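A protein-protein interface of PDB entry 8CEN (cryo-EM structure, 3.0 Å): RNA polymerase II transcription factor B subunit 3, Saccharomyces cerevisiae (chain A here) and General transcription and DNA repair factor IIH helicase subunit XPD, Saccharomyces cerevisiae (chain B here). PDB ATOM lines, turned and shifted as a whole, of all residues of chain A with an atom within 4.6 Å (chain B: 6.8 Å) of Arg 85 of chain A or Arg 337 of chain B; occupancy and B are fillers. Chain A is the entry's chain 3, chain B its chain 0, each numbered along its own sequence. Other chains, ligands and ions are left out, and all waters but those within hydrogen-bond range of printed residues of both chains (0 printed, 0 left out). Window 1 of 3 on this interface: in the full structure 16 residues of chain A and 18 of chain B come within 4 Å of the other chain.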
ATOM      1  N   VAL A  78      -1.417 -19.372 -23.462  1.00  0.00           N
ATOM      2  CA  VAL A  78      -1.504 -20.804 -23.729  1.00  0.00           C
ATOM      3  C   VAL A  78      -2.816 -21.367 -23.194  1.00  0.00           C
ATOM      4  O   VAL A  78      -3.474 -22.176 -23.860  1.00  0.00           O
ATOM      5  CB  VAL A  78      -0.279 -21.530 -23.144  1.00  0.00           C
ATOM      6  CG1 VAL A  78      -0.462 -23.039 -23.203  1.00  0.00           C
ATOM      7  CG2 VAL A  78       0.974 -21.123 -23.900  1.00  0.00           C
ATOM      8  N   GLU A  81      -5.521 -20.306 -25.496  1.00  0.00           N
ATOM      9  CA  GLU A  81      -5.390 -20.984 -26.781  1.00  0.00           C
ATOM     10  C   GLU A  81      -5.929 -22.407 -26.709  1.00  0.00           C
ATOM     11  O   GLU A  81      -6.654 -22.843 -27.609  1.00  0.00           O
ATOM     12  CB  GLU A  81      -3.923 -20.964 -27.227  1.00  0.00           C
ATOM     13  CG  GLU A  81      -3.649 -21.426 -28.664  1.00  0.00           C
ATOM     14  CD  GLU A  81      -3.535 -22.934 -28.811  1.00  0.00           C
ATOM     15  OE1 GLU A  81      -3.127 -23.600 -27.836  1.00  0.00           O
ATOM     16  OE2 GLU A  81      -3.856 -23.452 -29.901  1.00  0.00           O
ATOM     17  N   VAL A  82      -5.599 -23.144 -25.645  1.00  0.00           N
ATOM     18  CA  VAL A  82      -6.130 -24.501 -25.507  1.00  0.00           C
ATOM     19  C   VAL A  82      -7.630 -24.487 -25.214  1.00  0.00           C
ATOM     20  O   VAL A  82      -8.356 -25.384 -25.660  1.00  0.00           O
ATOM     21  CB  VAL A  82      -5.340 -25.302 -24.454  1.00  0.00           C
ATOM     22  CG1 VAL A  82      -5.686 -26.776 -24.538  1.00  0.00           C
ATOM     23  CG2 VAL A  82      -3.861 -25.178 -24.731  1.00  0.00           C
ATOM     24  N   ASP A  83      -8.131 -23.485 -24.483  1.00  0.00           N
ATOM     25  CA  ASP A  83      -9.578 -23.399 -24.281  1.00  0.00           C
ATOM     26  C   ASP A  83     -10.317 -23.119 -25.588  1.00  0.00           C
ATOM     27  O   ASP A  83     -11.369 -23.717 -25.854  1.00  0.00           O
ATOM     28  CB  ASP A  83      -9.905 -22.338 -23.235  1.00  0.00           C
ATOM     29  CG  ASP A  83      -9.460 -22.740 -21.842  1.00  0.00           C
ATOM     30  OD1 ASP A  83      -9.423 -23.955 -21.556  1.00  0.00           O
ATOM     31  OD2 ASP A  83      -9.150 -21.842 -21.030  1.00  0.00           O
ATOM     32  N   ILE A  84      -9.775 -22.229 -26.426  1.00  0.00           N
ATOM     33  CA  ILE A  84     -10.356 -21.979 -27.743  1.00  0.00           C
ATOM     34  C   ILE A  84     -10.251 -23.224 -28.620  1.00  0.00           C
ATOM     35  O   ILE A  84     -11.170 -23.544 -29.387  1.00  0.00           O
ATOM     36  CB  ILE A  84      -9.678 -20.751 -28.384  1.00  0.00           C
ATOM     37  CG1 ILE A  84     -10.137 -19.470 -27.683  1.00  0.00           C
ATOM     38  CG2 ILE A  84      -9.954 -20.663 -29.873  1.00  0.00           C
ATOM     39  CD1 ILE A  84      -9.221 -18.291 -27.904  1.00  0.00           C
ATOM     40  N   ARG A  85      -9.144 -23.961 -28.494  1.00  0.00           N
ATOM     41  CA  ARG A  85      -8.973 -25.204 -29.239  1.00  0.00           C
ATOM     42  C   ARG A  85     -10.014 -26.241 -28.835  1.00  0.00           C
ATOM     43  O   ARG A  85     -10.535 -26.969 -29.685  1.00  0.00           O
ATOM     44  CB  ARG A  85      -7.558 -25.741 -29.021  1.00  0.00           C
ATOM     45  CG  ARG A  85      -7.256 -27.051 -29.726  1.00  0.00           C
ATOM     46  CD  ARG A  85      -5.760 -27.303 -29.772  1.00  0.00           C
ATOM     47  NE  ARG A  85      -5.036 -26.162 -30.321  1.00  0.00           N
ATOM     48  CZ  ARG A  85      -4.777 -25.990 -31.610  1.00  0.00           C
ATOM     49  NH1 ARG A  85      -5.159 -26.875 -32.515  1.00  0.00           N
ATOM     50  NH2 ARG A  85      -4.117 -24.904 -32.000  1.00  0.00           N
ATOM     51  N   LYS A  86     -10.329 -26.317 -27.540  1.00  0.00           N
ATOM     52  CA  LYS A  86     -11.406 -27.189 -27.080  1.00  0.00           C
ATOM     53  C   LYS A  86     -12.756 -26.736 -27.624  1.00  0.00           C
ATOM     54  O   LYS A  86     -13.553 -27.559 -28.095  1.00  0.00           O
ATOM     55  CB  LYS A  86     -11.434 -27.223 -25.552  1.00  0.00           C
ATOM     56  CG  LYS A  86     -12.351 -28.288 -24.968  1.00  0.00           C
ATOM     57  CD  LYS A  86     -11.859 -28.771 -23.609  1.00  0.00           C
ATOM     58  CE  LYS A  86     -11.513 -27.608 -22.689  1.00  0.00           C
ATOM     59  NZ  LYS A  86     -10.532 -27.997 -21.638  1.00  0.00           N
ATOM     60  N   ARG A  87     -13.022 -25.426 -27.581  1.00  0.00           N
ATOM     61  CA  ARG A  87     -14.287 -24.889 -28.078  1.00  0.00           C
ATOM     62  C   ARG A  87     -14.441 -25.035 -29.587  1.00  0.00           C
ATOM     63  O   ARG A  87     -15.562 -24.933 -30.094  1.00  0.00           O
ATOM     64  CB  ARG A  87     -14.429 -23.415 -27.691  1.00  0.00           C
ATOM     65  CG  ARG A  87     -14.560 -23.166 -26.197  1.00  0.00           C
ATOM     66  CD  ARG A  87     -15.228 -21.827 -25.894  1.00  0.00           C
ATOM     67  NE  ARG A  87     -14.410 -20.685 -26.286  1.00  0.00           N
ATOM     68  CZ  ARG A  87     -14.604 -19.957 -27.377  1.00  0.00           C
ATOM     69  NH1 ARG A  87     -15.587 -20.225 -28.221  1.00  0.00           N
ATOM     70  NH2 ARG A  87     -13.793 -18.934 -27.628  1.00  0.00           N
ATOM     71  N   VAL A  88     -13.347 -25.235 -30.314  1.00  0.00           N
ATOM     72  CA  VAL A  88     -13.428 -25.525 -31.744  1.00  0.00           C
ATOM     73  C   VAL A  88     -13.550 -27.023 -31.998  1.00  0.00           C
ATOM     74  O   VAL A  88     -14.410 -27.471 -32.763  1.00  0.00           O
ATOM     75  CB  VAL A  88     -12.207 -24.922 -32.473  1.00  0.00           C
ATOM     76  CG1 VAL A  88     -12.104 -25.461 -33.893  1.00  0.00           C
ATOM     77  CG2 VAL A  88     -12.297 -23.408 -32.489  1.00  0.00           C
ATOM     78  N   PHE A  89     -12.709 -27.826 -31.342  1.00  0.00           N
ATOM     79  CA  PHE A  89     -12.666 -29.263 -31.575  1.00  0.00           C
ATOM     80  C   PHE A  89     -13.857 -30.004 -30.984  1.00  0.00           C
ATOM     81  O   PHE A  89     -14.027 -31.190 -31.288  1.00  0.00           O
ATOM     82  CB  PHE A  89     -11.372 -29.845 -31.005  1.00  0.00           C
ATOM     83  CG  PHE A  89     -10.253 -29.930 -32.004  1.00  0.00           C
ATOM     84  CD1 PHE A  89     -10.172 -30.996 -32.886  1.00  0.00           C
ATOM     85  CD2 PHE A  89      -9.279 -28.946 -32.056  1.00  0.00           C
ATOM     86  CE1 PHE A  89      -9.142 -31.075 -33.806  1.00  0.00           C
ATOM     87  CE2 PHE A  89      -8.247 -29.020 -32.971  1.00  0.00           C
ATOM     88  CZ  PHE A  89      -8.177 -30.085 -33.848  1.00  0.00           C
ATOM     89  N   GLU A 114      -6.586 -24.884 -37.660  1.00  0.00           N
ATOM     90  CA  GLU A 114      -5.594 -24.018 -37.025  1.00  0.00           C
ATOM     91  C   GLU A 114      -5.768 -22.555 -37.419  1.00  0.00           C
ATOM     92  O   GLU A 114      -5.513 -21.670 -36.594  1.00  0.00           O
ATOM     93  CB  GLU A 114      -4.176 -24.499 -37.332  1.00  0.00           C
ATOM     94  CG  GLU A 114      -3.911 -25.959 -37.004  1.00  0.00           C
ATOM     95  CD  GLU A 114      -4.153 -26.288 -35.543  1.00  0.00           C
ATOM     96  OE1 GLU A 114      -3.835 -25.445 -34.677  1.00  0.00           O
ATOM     97  OE2 GLU A 114      -4.666 -27.391 -35.259  1.00  0.00           O
ATOM     98  N   ILE A 117      -8.665 -21.309 -35.268  1.00  0.00           N
ATOM     99  CA  ILE A 117      -8.221 -21.232 -33.878  1.00  0.00           C
ATOM    100  C   ILE A 117      -7.330 -20.011 -33.664  1.00  0.00           C
ATOM    101  O   ILE A 117      -7.484 -19.280 -32.677  1.00  0.00           O
ATOM    102  CB  ILE A 117      -7.518 -22.545 -33.480  1.00  0.00           C
ATOM    103  CG1 ILE A 117      -8.558 -23.642 -33.244  1.00  0.00           C
ATOM    104  CG2 ILE A 117      -6.651 -22.360 -32.241  1.00  0.00           C
ATOM    105  CD1 ILE A 117      -7.974 -24.959 -32.805  1.00  0.00           C
ATOM    106  N   ASN B 324      -1.033 -29.419 -38.829  1.00  0.00           N
ATOM    107  CA  ASN B 324      -1.191 -28.694 -37.573  1.00  0.00           C
ATOM    108  C   ASN B 324      -0.020 -27.754 -37.324  1.00  0.00           C
ATOM    109  O   ASN B 324      -0.192 -26.704 -36.696  1.00  0.00           O
ATOM    110  CB  ASN B 324      -1.321 -29.664 -36.399  1.00  0.00           C
ATOM    111  CG  ASN B 324      -2.556 -30.529 -36.484  1.00  0.00           C
ATOM    112  OD1 ASN B 324      -2.463 -31.746 -36.631  1.00  0.00           O
ATOM    113  ND2 ASN B 324      -3.724 -29.905 -36.391  1.00  0.00           N
ATOM    114  N   ILE B 325       1.169 -28.118 -37.795  1.00  0.00           N
ATOM    115  CA  ILE B 325       2.394 -27.378 -37.532  1.00  0.00           C
ATOM    116  C   ILE B 325       3.027 -26.854 -38.822  1.00  0.00           C
ATOM    117  O   ILE B 325       4.188 -26.462 -38.824  1.00  0.00           O
ATOM    118  CB  ILE B 325       3.387 -28.243 -36.732  1.00  0.00           C
ATOM    119  CG1 ILE B 325       3.779 -29.482 -37.540  1.00  0.00           C
ATOM    120  CG2 ILE B 325       2.786 -28.658 -35.407  1.00  0.00           C
ATOM    121  CD1 ILE B 325       4.917 -30.267 -36.938  1.00  0.00           C
ATOM    122  N   HIS B 330       1.391 -21.469 -36.245  1.00  0.00           N
ATOM    123  CA  HIS B 330       0.733 -22.675 -35.753  1.00  0.00           C
ATOM    124  C   HIS B 330       1.725 -23.590 -35.048  1.00  0.00           C
ATOM    125  O   HIS B 330       1.426 -24.138 -33.979  1.00  0.00           O
ATOM    126  CB  HIS B 330       0.060 -23.415 -36.909  1.00  0.00           C
ATOM    127  CG  HIS B 330      -0.976 -22.609 -37.631  1.00  0.00           C
ATOM    128  ND1 HIS B 330      -1.575 -23.046 -38.792  1.00  0.00           N
ATOM    129  CD2 HIS B 330      -1.525 -21.403 -37.356  1.00  0.00           C
ATOM    130  CE1 HIS B 330      -2.441 -22.139 -39.207  1.00  0.00           C
ATOM    131  NE2 HIS B 330      -2.432 -21.133 -38.352  1.00  0.00           N
ATOM    132  N   PHE B 331       2.920 -23.751 -35.622  1.00  0.00           N
ATOM    133  CA  PHE B 331       3.934 -24.590 -34.994  1.00  0.00           C
ATOM    134  C   PHE B 331       4.474 -23.957 -33.717  1.00  0.00           C
ATOM    135  O   PHE B 331       4.788 -24.676 -32.763  1.00  0.00           O
ATOM    136  CB  PHE B 331       5.066 -24.877 -35.980  1.00  0.00           C
ATOM    137  CG  PHE B 331       6.257 -25.545 -35.355  1.00  0.00           C
ATOM    138  CD1 PHE B 331       6.173 -26.852 -34.901  1.00  0.00           C
ATOM    139  CD2 PHE B 331       7.459 -24.872 -35.225  1.00  0.00           C
ATOM    140  CE1 PHE B 331       7.262 -27.471 -34.325  1.00  0.00           C
ATOM    141  CE2 PHE B 331       8.552 -25.488 -34.651  1.00  0.00           C
ATOM    142  CZ  PHE B 331       8.453 -26.789 -34.200  1.00  0.00           C
ATOM    143  N   VAL B 332       4.575 -22.624 -33.672  1.00  0.00           N
ATOM    144  CA  VAL B 332       4.999 -21.956 -32.442  1.00  0.00           C
ATOM    145  C   VAL B 332       3.962 -22.146 -31.337  1.00  0.00           C
ATOM    146  O   VAL B 332       4.316 -22.414 -30.182  1.00  0.00           O
ATOM    147  CB  VAL B 332       5.293 -20.467 -32.708  1.00  0.00           C
ATOM    148  CG1 VAL B 332       5.557 -19.728 -31.409  1.00  0.00           C
ATOM    149  CG2 VAL B 332       6.508 -20.326 -33.607  1.00  0.00           C
ATOM    150  N   SER B 333       2.671 -22.035 -31.671  1.00  0.00           N
ATOM    151  CA  SER B 333       1.623 -22.282 -30.680  1.00  0.00           C
ATOM    152  C   SER B 333       1.624 -23.735 -30.212  1.00  0.00           C
ATOM    153  O   SER B 333       1.442 -24.012 -29.018  1.00  0.00           O
ATOM    154  CB  SER B 333       0.258 -21.908 -31.257  1.00  0.00           C
ATOM    155  OG  SER B 333       0.198 -20.529 -31.574  1.00  0.00           O
ATOM    156  N   PHE B 334       1.831 -24.670 -31.146  1.00  0.00           N
ATOM    157  CA  PHE B 334       1.922 -26.092 -30.817  1.00  0.00           C
ATOM    158  C   PHE B 334       3.076 -26.360 -29.855  1.00  0.00           C
ATOM    159  O   PHE B 334       2.910 -27.041 -28.834  1.00  0.00           O
ATOM    160  CB  PHE B 334       2.085 -26.879 -32.123  1.00  0.00           C
ATOM    161  CG  PHE B 334       2.247 -28.365 -31.953  1.00  0.00           C
ATOM    162  CD1 PHE B 334       1.137 -29.191 -31.949  1.00  0.00           C
ATOM    163  CD2 PHE B 334       3.506 -28.944 -31.874  1.00  0.00           C
ATOM    164  CE1 PHE B 334       1.273 -30.557 -31.825  1.00  0.00           C
ATOM    165  CE2 PHE B 334       3.649 -30.311 -31.745  1.00  0.00           C
ATOM    166  CZ  PHE B 334       2.530 -31.118 -31.723  1.00  0.00           C
ATOM    167  N   LEU B 335       4.250 -25.801 -30.162  1.00  0.00           N
ATOM    168  CA  LEU B 335       5.421 -25.967 -29.309  1.00  0.00           C
ATOM    169  C   LEU B 335       5.212 -25.330 -27.942  1.00  0.00           C
ATOM    170  O   LEU B 335       5.603 -25.904 -26.919  1.00  0.00           O
ATOM    171  CB  LEU B 335       6.645 -25.368 -30.001  1.00  0.00           C
ATOM    172  CG  LEU B 335       8.016 -25.935 -29.644  1.00  0.00           C
ATOM    173  CD1 LEU B 335       8.143 -27.357 -30.140  1.00  0.00           C
ATOM    174  CD2 LEU B 335       9.100 -25.065 -30.251  1.00  0.00           C
ATOM    175  N   LYS B 336       4.590 -24.149 -27.904  1.00  0.00           N
ATOM    176  CA  LYS B 336       4.372 -23.455 -26.638  1.00  0.00           C
ATOM    177  C   LYS B 336       3.412 -24.222 -25.738  1.00  0.00           C
ATOM    178  O   LYS B 336       3.654 -24.347 -24.530  1.00  0.00           O
ATOM    179  CB  LYS B 336       3.851 -22.043 -26.902  1.00  0.00           C
ATOM    180  CG  LYS B 336       4.300 -21.016 -25.878  1.00  0.00           C
ATOM    181  CD  LYS B 336       4.112 -19.599 -26.395  1.00  0.00           C
ATOM    182  CE  LYS B 336       4.801 -19.402 -27.736  1.00  0.00           C
ATOM    183  NZ  LYS B 336       4.699 -17.996 -28.214  1.00  0.00           N
ATOM    184  N   ARG B 337       2.331 -24.766 -26.304  1.00  0.00           N
ATOM    185  CA  ARG B 337       1.411 -25.525 -25.466  1.00  0.00           C
ATOM    186  C   ARG B 337       1.991 -26.881 -25.073  1.00  0.00           C
ATOM    187  O   ARG B 337       1.691 -27.380 -23.982  1.00  0.00           O
ATOM    188  CB  ARG B 337       0.047 -25.664 -26.151  1.00  0.00           C
ATOM    189  CG  ARG B 337      -0.023 -26.560 -27.369  1.00  0.00           C
ATOM    190  CD  ARG B 337      -1.463 -26.617 -27.865  1.00  0.00           C
ATOM    191  NE  ARG B 337      -1.629 -27.459 -29.044  1.00  0.00           N
ATOM    192  CZ  ARG B 337      -1.623 -27.009 -30.290  1.00  0.00           C
ATOM    193  NH1 ARG B 337      -1.459 -25.725 -30.561  1.00  0.00           N
ATOM    194  NH2 ARG B 337      -1.793 -27.868 -31.290  1.00  0.00           N
ATOM    195  N   LEU B 338       2.860 -27.466 -25.907  1.00  0.00           N
ATOM    196  CA  LEU B 338       3.570 -28.678 -25.498  1.00  0.00           C
ATOM    197  C   LEU B 338       4.514 -28.406 -24.328  1.00  0.00           C
ATOM    198  O   LEU B 338       4.579 -29.192 -23.372  1.00  0.00           O
ATOM    199  CB  LEU B 338       4.341 -29.256 -26.684  1.00  0.00           C
ATOM    200  CG  LEU B 338       5.281 -30.426 -26.386  1.00  0.00           C
ATOM    201  CD1 LEU B 338       4.492 -31.667 -26.004  1.00  0.00           C
ATOM    202  CD2 LEU B 338       6.189 -30.703 -27.573  1.00  0.00           C
ATOM    203  N   ILE B 339       5.248 -27.291 -24.385  1.00  0.00           N
ATOM    204  CA  ILE B 339       6.162 -26.930 -23.304  1.00  0.00           C
ATOM    205  C   ILE B 339       5.387 -26.624 -22.026  1.00  0.00           C
ATOM    206  O   ILE B 339       5.806 -27.003 -20.923  1.00  0.00           O
ATOM    207  CB  ILE B 339       7.054 -25.752 -23.742  1.00  0.00           C
ATOM    208  CG1 ILE B 339       8.011 -26.196 -24.846  1.00  0.00           C
ATOM    209  CG2 ILE B 339       7.861 -25.206 -22.580  1.00  0.00           C
ATOM    210  CD1 ILE B 339       8.632 -25.051 -25.610  1.00  0.00           C
ATOM    211  N   GLU B 340       4.233 -25.963 -22.151  1.00  0.00           N
ATOM    212  CA  GLU B 340       3.406 -25.700 -20.977  1.00  0.00           C
ATOM    213  C   GLU B 340       2.843 -26.991 -20.388  1.00  0.00           C
ATOM    214  O   GLU B 340       2.738 -27.122 -19.162  1.00  0.00           O
ATOM    215  CB  GLU B 340       2.285 -24.729 -21.332  1.00  0.00           C
ATOM    216  CG  GLU B 340       2.751 -23.289 -21.420  1.00  0.00           C
ATOM    217  CD  GLU B 340       3.481 -22.841 -20.170  1.00  0.00           C
ATOM    218  OE1 GLU B 340       2.922 -22.996 -19.064  1.00  0.00           O
ATOM    219  OE2 GLU B 340       4.617 -22.339 -20.293  1.00  0.00           O
ATOM    220  N   TYR B 341       2.488 -27.958 -21.242  1.00  0.00           N
ATOM    221  CA  TYR B 341       2.064 -29.263 -20.744  1.00  0.00           C
ATOM    222  C   TYR B 341       3.190 -29.960 -19.990  1.00  0.00           C
ATOM    223  O   TYR B 341       2.952 -30.613 -18.968  1.00  0.00           O
ATOM    224  CB  TYR B 341       1.574 -30.136 -21.897  1.00  0.00           C
ATOM    225  CG  TYR B 341       1.237 -31.552 -21.484  1.00  0.00           C
ATOM    226  CD1 TYR B 341       0.035 -31.840 -20.853  1.00  0.00           C
ATOM    227  CD2 TYR B 341       2.120 -32.598 -21.723  1.00  0.00           C
ATOM    228  CE1 TYR B 341      -0.279 -33.128 -20.472  1.00  0.00           C
ATOM    229  CE2 TYR B 341       1.811 -33.889 -21.347  1.00  0.00           C
ATOM    230  CZ  TYR B 341       0.613 -34.147 -20.721  1.00  0.00           C
ATOM    231  OH  TYR B 341       0.304 -35.432 -20.343  1.00  0.00           O
ATOM    232  N   LEU B 342       4.423 -29.842 -20.491  1.00  0.00           N
ATOM    233  CA  LEU B 342       5.571 -30.408 -19.784  1.00  0.00           C
ATOM    234  C   LEU B 342       5.780 -29.731 -18.432  1.00  0.00           C
ATOM    235  O   LEU B 342       6.125 -30.391 -17.439  1.00  0.00           O
ATOM    236  CB  LEU B 342       6.824 -30.288 -20.649  1.00  0.00           C
ATOM    237  CG  LEU B 342       6.875 -31.185 -21.887  1.00  0.00           C
ATOM    238  CD1 LEU B 342       8.202 -31.030 -22.606  1.00  0.00           C
ATOM    239  CD2 LEU B 342       6.631 -32.637 -21.511  1.00  0.00           C
ATOM    240  N   LEU B 363      -1.603 -36.244 -22.849  1.00  0.00           N
ATOM    241  CA  LEU B 363      -1.335 -35.016 -23.590  1.00  0.00           C
ATOM    242  C   LEU B 363      -2.447 -34.713 -24.587  1.00  0.00           C
ATOM    243  O   LEU B 363      -2.819 -33.551 -24.776  1.00  0.00           O
ATOM    244  CB  LEU B 363       0.016 -35.136 -24.295  1.00  0.00           C
ATOM    245  CG  LEU B 363       0.431 -34.154 -25.391  1.00  0.00           C
ATOM    246  CD1 LEU B 363       0.490 -32.736 -24.873  1.00  0.00           C
ATOM    247  CD2 LEU B 363       1.776 -34.561 -25.941  1.00  0.00           C
ATOM    248  N   THR B 367      -4.498 -31.364 -23.921  1.00  0.00           N
ATOM    249  CA  THR B 367      -3.887 -30.318 -24.725  1.00  0.00           C
ATOM    250  C   THR B 367      -4.326 -30.383 -26.190  1.00  0.00           C
ATOM    251  O   THR B 367      -4.220 -29.371 -26.897  1.00  0.00           O
ATOM    252  CB  THR B 367      -2.350 -30.422 -24.592  1.00  0.00           C
ATOM    253  OG1 THR B 367      -1.999 -30.272 -23.212  1.00  0.00           O
ATOM    254  CG2 THR B 367      -1.590 -29.329 -25.336  1.00  0.00           C
ATOM    255  N   PHE B 368      -4.914 -31.506 -26.625  1.00  0.00           N
ATOM    256  CA  PHE B 368      -5.292 -31.773 -28.021  1.00  0.00           C
ATOM    257  C   PHE B 368      -4.073 -31.722 -28.941  1.00  0.00           C
ATOM    258  O   PHE B 368      -4.083 -31.090 -29.999  1.00  0.00           O
ATOM    259  CB  PHE B 368      -6.403 -30.836 -28.514  1.00  0.00           C
ATOM    260  CG  PHE B 368      -7.599 -30.788 -27.610  1.00  0.00           C
ATOM    261  CD1 PHE B 368      -8.576 -31.768 -27.683  1.00  0.00           C
ATOM    262  CD2 PHE B 368      -7.746 -29.767 -26.686  1.00  0.00           C
ATOM    263  CE1 PHE B 368      -9.679 -31.729 -26.853  1.00  0.00           C
ATOM    264  CE2 PHE B 368      -8.843 -29.723 -25.851  1.00  0.00           C
ATOM    265  CZ  PHE B 368      -9.812 -30.705 -25.936  1.00  0.00           C
ATOM    266  N   ILE B 369      -3.013 -32.403 -28.518  1.00  0.00           N
ATOM    267  CA  ILE B 369      -1.815 -32.615 -29.320  1.00  0.00           C
ATOM    268  C   ILE B 369      -1.754 -34.092 -29.683  1.00  0.00           C
ATOM    269  O   ILE B 369      -1.815 -34.956 -28.801  1.00  0.00           O
ATOM    270  CB  ILE B 369      -0.549 -32.168 -28.567  1.00  0.00           C
ATOM    271  CG1 ILE B 369      -0.400 -30.646 -28.629  1.00  0.00           C
ATOM    272  CG2 ILE B 369       0.685 -32.851 -29.123  1.00  0.00           C
ATOM    273  CD1 ILE B 369       0.888 -30.132 -28.022  1.00  0.00           C
ATOM    274  N   GLU B 370      -1.651 -34.380 -30.976  1.00  0.00           N
ATOM    275  CA  GLU B 370      -1.636 -35.754 -31.450  1.00  0.00           C
ATOM    276  C   GLU B 370      -0.203 -36.262 -31.609  1.00  0.00           C
ATOM    277  O   GLU B 370       0.771 -35.519 -31.475  1.00  0.00           O
ATOM    278  CB  GLU B 370      -2.399 -35.871 -32.772  1.00  0.00           C
ATOM    279  CG  GLU B 370      -3.927 -35.895 -32.650  1.00  0.00           C
ATOM    280  CD  GLU B 370      -4.509 -37.250 -32.252  1.00  0.00           C
ATOM    281  OE1 GLU B 370      -3.818 -38.068 -31.611  1.00  0.00           O
ATOM    282  OE2 GLU B 370      -5.685 -37.497 -32.593  1.00  0.00           O
ATOM    283  N   PRO B 373       1.668 -35.002 -35.431  1.00  0.00           N
ATOM    284  CA  PRO B 373       2.387 -33.713 -35.445  1.00  0.00           C
ATOM    285  C   PRO B 373       3.610 -33.685 -34.545  1.00  0.00           C
ATOM    286  O   PRO B 373       4.546 -32.922 -34.811  1.00  0.00           O
ATOM    287  CB  PRO B 373       1.323 -32.708 -34.978  1.00  0.00           C
ATOM    288  CG  PRO B 373       0.309 -33.521 -34.281  1.00  0.00           C
ATOM    289  CD  PRO B 373       0.256 -34.789 -35.058  1.00  0.00           C
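Of the 21 printed residues of chain B, 7 touch a printed residue of chain A.
Hydrophobic or aromatic side chains of chain B that line the printed part of chain A: His 330 and Phe 368.
Of the 12 printed residues of chain A, 6 touch a printed residue of chain B.
Hydrophobic or aromatic side chains of chain A within 4 Å of the printed part of chain B: Val 78 and Val 82.
Among the printed residues, Asp or Glu carboxylates within 4 Å of a Lys or Arg side-chain nitrogen of the other chain: Glu 81 of chain A with Arg 337 of chain B (3.4 Å).
Arg 85 of chain A touches three residues of chain B.
Arg 337 of chain B touches just these residues of chain A: Val 78 (3.8 Å), Glu 81 (3.4 Å) and Arg 85 (3.1 Å).
Of the printed residues of chain A, Thr 367 of chain B touches Val 82 (3.8 Å) and Arg 85 (3.9 Å).
Printed residues of chain A within 4 Å of Glu 340 of chain B: Val 78 (3.7 Å).
Of the printed residues of chain B, Val 78 of chain A touches Lys 336 (3.9 Å), Arg 337 (3.8 Å) and Glu 340 (3.7 Å).
Printed residues of chain B within 4 Å of Val 82 of chain A: Thr 367.
Ile 84 of chain A touches none of the printed residues of chain B.
N of Phe 368 of chain B is in hydrogen-bond range of O of Leu 363 of chain B (3.5 Å).
OE2 of Glu 81 of chain A is in salt-bridge range of NH2 of Arg 85 of chain A, 2.6 Å away.
The side-chain carboxylate (OE1) of Glu 114 of chain A lies within salt-bridge range of the guanidinium group (NH2) of Arg 85 of chain A (2.7 Å).
NH1 of Arg 337 of chain B is in salt-bridge range of OE2 of Glu 81 of chain A, at 3.4 Å.
The guanidinium group of Arg 85 of chain A lies close to the guanidinium group of Arg 337 of chain B.
ND2 of Asn 324 of chain B is in hydrogen-bond range of OE2 of Glu 114 of chain A (2.9 Å).
Among the printed residues, merely in contact across the chains: Glu 114 of chain A with His 330 of chain B (3.3 Å), Lys 86 of chain A with Phe 368 of chain B (3.6 Å), Val 78 of chain A with Glu 340 of chain B (3.7 Å), Val 82 of chain A with Thr 367 of chain B (3.8 Å), Arg 85 of chain A with Phe 368 of chain B (3.8 Å), Val 78 of chain A with Arg 337 of chain B (3.8 Å), Arg 85 of chain A with Thr 367 of chain B (3.9 Å) and Val 78 of chain A with Lys 336 of chain B (3.9 Å).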
